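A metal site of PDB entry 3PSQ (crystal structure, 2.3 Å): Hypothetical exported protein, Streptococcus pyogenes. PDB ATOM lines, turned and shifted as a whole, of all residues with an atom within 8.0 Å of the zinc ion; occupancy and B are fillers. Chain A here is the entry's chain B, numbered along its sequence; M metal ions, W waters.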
ATOM      1  N   ILE A  61      -1.489 -25.242 -24.264  1.00  0.00           N
ATOM      2  CA  ILE A  61      -0.089 -25.670 -24.246  1.00  0.00           C
ATOM      3  C   ILE A  61       0.865 -24.540 -23.902  1.00  0.00           C
ATOM      4  O   ILE A  61       1.810 -24.728 -23.126  1.00  0.00           O
ATOM      5  CB  ILE A  61       0.305 -26.400 -25.543  1.00  0.00           C
ATOM      6  CG1 ILE A  61      -0.564 -27.649 -25.703  1.00  0.00           C
ATOM      7  CG2 ILE A  61       1.773 -26.862 -25.510  1.00  0.00           C
ATOM      8  CD1 ILE A  61      -0.464 -28.289 -27.033  1.00  0.00           C
ATOM      9  N   ASN A  62       0.599 -23.356 -24.448  1.00  0.00           N
ATOM     10  CA  ASN A  62       1.492 -22.178 -24.339  1.00  0.00           C
ATOM     11  C   ASN A  62       0.741 -20.886 -23.952  1.00  0.00           C
ATOM     12  O   ASN A  62       1.174 -19.750 -24.312  1.00  0.00           O
ATOM     13  CB  ASN A  62       2.229 -21.948 -25.656  1.00  0.00           C
ATOM     14  CG  ASN A  62       3.168 -23.110 -25.988  1.00  0.00           C
ATOM     15  OD1 ASN A  62       3.975 -23.489 -25.163  1.00  0.00           O
ATOM     16  ND2 ASN A  62       3.017 -23.698 -27.147  1.00  0.00           N
ATOM     17  N   LEU A  71       5.200 -20.474 -21.678  1.00  0.00           N
ATOM     18  CA  LEU A  71       5.660 -21.823 -22.007  1.00  0.00           C
ATOM     19  C   LEU A  71       5.179 -22.863 -20.963  1.00  0.00           C
ATOM     20  O   LEU A  71       5.210 -24.056 -21.225  1.00  0.00           O
ATOM     21  CB  LEU A  71       7.197 -21.863 -22.235  1.00  0.00           C
ATOM     22  CG  LEU A  71       7.723 -21.061 -23.471  1.00  0.00           C
ATOM     23  CD1 LEU A  71       9.251 -21.010 -23.577  1.00  0.00           C
ATOM     24  CD2 LEU A  71       7.146 -21.546 -24.820  1.00  0.00           C
ATOM     25  N   SER A  72       4.707 -22.428 -19.790  1.00  0.00           N
ATOM     26  CA  SER A  72       4.163 -23.348 -18.754  1.00  0.00           C
ATOM     27  C   SER A  72       2.717 -23.714 -19.005  1.00  0.00           C
ATOM     28  O   SER A  72       2.155 -24.619 -18.381  1.00  0.00           O
ATOM     29  CB  SER A  72       4.191 -22.677 -17.394  1.00  0.00           C
ATOM     30  OG  SER A  72       5.474 -22.158 -17.172  1.00  0.00           O
ATOM     31  N   ALA A  94      -1.044 -31.256 -18.066  1.00  0.00           N
ATOM     32  CA  ALA A  94      -0.214 -30.075 -17.831  1.00  0.00           C
ATOM     33  C   ALA A  94       1.221 -30.462 -18.125  1.00  0.00           C
ATOM     34  O   ALA A  94       1.544 -31.653 -18.115  1.00  0.00           O
ATOM     35  CB  ALA A  94      -0.353 -29.575 -16.367  1.00  0.00           C
ATOM     36  N   HIS A  95       2.092 -29.472 -18.341  1.00  0.00           N
ATOM     37  CA  HIS A  95       3.498 -29.727 -18.671  1.00  0.00           C
ATOM     38  C   HIS A  95       4.260 -30.337 -17.509  1.00  0.00           C
ATOM     39  O   HIS A  95       4.084 -29.927 -16.354  1.00  0.00           O
ATOM     40  CB  HIS A  95       4.212 -28.416 -19.001  1.00  0.00           C
ATOM     41  CG  HIS A  95       3.845 -27.845 -20.333  1.00  0.00           C
ATOM     42  ND1 HIS A  95       4.331 -28.350 -21.517  1.00  0.00           N
ATOM     43  CD2 HIS A  95       3.081 -26.775 -20.672  1.00  0.00           C
ATOM     44  CE1 HIS A  95       3.846 -27.639 -22.525  1.00  0.00           C
ATOM     45  NE2 HIS A  95       3.092 -26.673 -22.042  1.00  0.00           N
ATOM     46  N   HIS A  96       5.142 -31.280 -17.838  1.00  0.00           N
ATOM     47  CA  HIS A  96       6.201 -31.654 -16.907  1.00  0.00           C
ATOM     48  C   HIS A  96       7.326 -30.626 -17.042  1.00  0.00           C
ATOM     49  O   HIS A  96       8.191 -30.741 -17.896  1.00  0.00           O
ATOM     50  CB  HIS A  96       6.700 -33.091 -17.145  1.00  0.00           C
ATOM     51  CG  HIS A  96       7.891 -33.467 -16.313  1.00  0.00           C
ATOM     52  ND1 HIS A  96       8.604 -34.628 -16.515  1.00  0.00           N
ATOM     53  CD2 HIS A  96       8.534 -32.806 -15.314  1.00  0.00           C
ATOM     54  CE1 HIS A  96       9.602 -34.682 -15.649  1.00  0.00           C
ATOM     55  NE2 HIS A  96       9.587 -33.582 -14.925  1.00  0.00           N
ATOM     56  N   MET A  97       7.282 -29.606 -16.210  1.00  0.00           N
ATOM     57  CA  MET A  97       8.303 -28.580 -16.261  1.00  0.00           C
ATOM     58  C   MET A  97       9.469 -28.980 -15.367  1.00  0.00           C
ATOM     59  O   MET A  97       9.266 -29.628 -14.327  1.00  0.00           O
ATOM     60  CB  MET A  97       7.741 -27.235 -15.717  1.00  0.00           C
ATOM     61  CG  MET A  97       6.539 -26.646 -16.485  1.00  0.00           C
ATOM     62  SD  MET A  97       6.948 -26.019 -18.130  1.00  0.00           S
ATOM     63  CE  MET A  97       8.042 -24.649 -17.771  1.00  0.00           C
ATOM     64  N   ALA A  98      10.672 -28.552 -15.759  1.00  0.00           N
ATOM     65  CA  ALA A  98      11.787 -28.445 -14.824  1.00  0.00           C
ATOM     66  C   ALA A  98      11.336 -27.668 -13.580  1.00  0.00           C
ATOM     67  O   ALA A  98      10.728 -26.611 -13.703  1.00  0.00           O
ATOM     68  CB  ALA A  98      12.941 -27.747 -15.503  1.00  0.00           C
ATOM     69  N   THR A 189       0.997 -35.854 -17.776  1.00  0.00           N
ATOM     70  CA  THR A 189       2.027 -34.888 -18.195  1.00  0.00           C
ATOM     71  C   THR A 189       1.942 -34.699 -19.722  1.00  0.00           C
ATOM     72  O   THR A 189       1.201 -35.424 -20.419  1.00  0.00           O
ATOM     73  CB  THR A 189       3.451 -35.337 -17.826  1.00  0.00           C
ATOM     74  OG1 THR A 189       3.755 -36.557 -18.504  1.00  0.00           O
ATOM     75  CG2 THR A 189       3.608 -35.536 -16.304  1.00  0.00           C
ATOM     76  N   CYS A 190       2.706 -33.716 -20.212  1.00  0.00           N
ATOM     77  CA  CYS A 190       2.693 -33.289 -21.620  1.00  0.00           C
ATOM     78  C   CYS A 190       3.261 -34.265 -22.659  1.00  0.00           C
ATOM     79  O   CYS A 190       3.988 -35.257 -22.323  1.00  0.00           O
ATOM     80  CB  CYS A 190       3.451 -31.985 -21.771  1.00  0.00           C
ATOM     81  SG  CYS A 190       5.087 -32.161 -21.167  1.00  0.00           S
ATOM     82  N   GLU A 191       2.932 -33.950 -23.919  1.00  0.00           N
ATOM     83  CA  GLU A 191       3.433 -34.674 -25.110  1.00  0.00           C
ATOM     84  C   GLU A 191       4.785 -34.130 -25.571  1.00  0.00           C
ATOM     85  O   GLU A 191       5.547 -34.831 -26.231  1.00  0.00           O
ATOM     86  CB  GLU A 191       2.460 -34.540 -26.318  1.00  0.00           C
ATOM     87  CG  GLU A 191       0.957 -34.721 -26.020  1.00  0.00           C
ATOM     88  CD  GLU A 191       0.135 -34.947 -27.314  1.00  0.00           C
ATOM     89  OE1 GLU A 191       0.712 -34.936 -28.426  1.00  0.00           O
ATOM     90  OE2 GLU A 191      -1.107 -35.139 -27.223  1.00  0.00           O
ATOM     91  N   ASP A 192       5.066 -32.881 -25.242  1.00  0.00           N
ATOM     92  CA  ASP A 192       6.266 -32.177 -25.726  1.00  0.00           C
ATOM     93  C   ASP A 192       7.523 -32.452 -24.885  1.00  0.00           C
ATOM     94  O   ASP A 192       8.631 -32.018 -25.238  1.00  0.00           O
ATOM     95  CB  ASP A 192       5.978 -30.676 -25.746  1.00  0.00           C
ATOM     96  CG  ASP A 192       5.482 -30.172 -24.391  1.00  0.00           C
ATOM     97  OD1 ASP A 192       6.342 -29.932 -23.530  1.00  0.00           O
ATOM     98  OD2 ASP A 192       4.243 -30.057 -24.184  1.00  0.00           O
ATOM     99  N   MET A 193       7.367 -33.124 -23.742  1.00  0.00           N
ATOM    100  CA  MET A 193       8.508 -33.374 -22.861  1.00  0.00           C
ATOM    101  C   MET A 193       8.258 -34.747 -22.251  1.00  0.00           C
ATOM    102  O   MET A 193       7.746 -34.885 -21.126  1.00  0.00           O
ATOM    103  CB  MET A 193       8.694 -32.281 -21.778  1.00  0.00           C
ATOM    104  CG  MET A 193      10.060 -32.315 -21.046  1.00  0.00           C
ATOM    105  SD  MET A 193      10.726 -33.978 -20.626  1.00  0.00           S
ATOM    106  CE  MET A 193      10.173 -34.225 -18.938  1.00  0.00           C
ATOM    107  N   THR A 194       8.521 -35.765 -23.071  1.00  0.00           N
ATOM    108  CA  THR A 194       8.173 -37.144 -22.738  1.00  0.00           C
ATOM    109  C   THR A 194       9.343 -38.076 -22.427  1.00  0.00           C
ATOM    110  O   THR A 194       9.182 -39.297 -22.423  1.00  0.00           O
ATOM    111  CB  THR A 194       7.333 -37.784 -23.862  1.00  0.00           C
ATOM    112  OG1 THR A 194       6.127 -37.042 -24.040  1.00  0.00           O
ATOM    113  CG2 THR A 194       6.993 -39.229 -23.517  1.00  0.00           C
HETATM  114 ZN    ZN M   1       5.644 -29.959 -21.774  1.00  0.00          ZN
HETATM  115  O   HOH W   1       7.349 -29.168 -20.783  1.00  0.00           O
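CB of Met 193 touches the zinc ion, at 3.8 Å.
Of the 15 residues printed, 4 come within 4 Å of the zinc ion.
The zinc ion is bound by the side-chain carboxylate (OD1) of Asp 192, a ring nitrogen (ND1) of His 95, water W1 and the side-chain sulfur (SG) of Cys 190.
The zinc ion has four donor atoms within binding distance.
Slightly farther from the zinc ion lies OD2 of Asp 192 (2.8 Å).
O of Cys 190 lies within hydrogen-bond range of OG1 of Thr 194 (3.3 Å).
O of Ile 61 is in hydrogen-bond range of NE2 of His 95 (2.6 Å).
SG of Cys 190 sits close to N of His 96, 3.4 Å away.
N of Cys 190 lies within hydrogen-bond range of O of Ala 94, at 3.2 Å.
A ring nitrogen (NE2) of His 95 is in hydrogen-bond range of the backbone carbonyl oxygen of Leu 71, at 3.5 Å.
The backbone NH (N) of Met 193 sits close to the side-chain sulfur (SG) of Cys 190.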
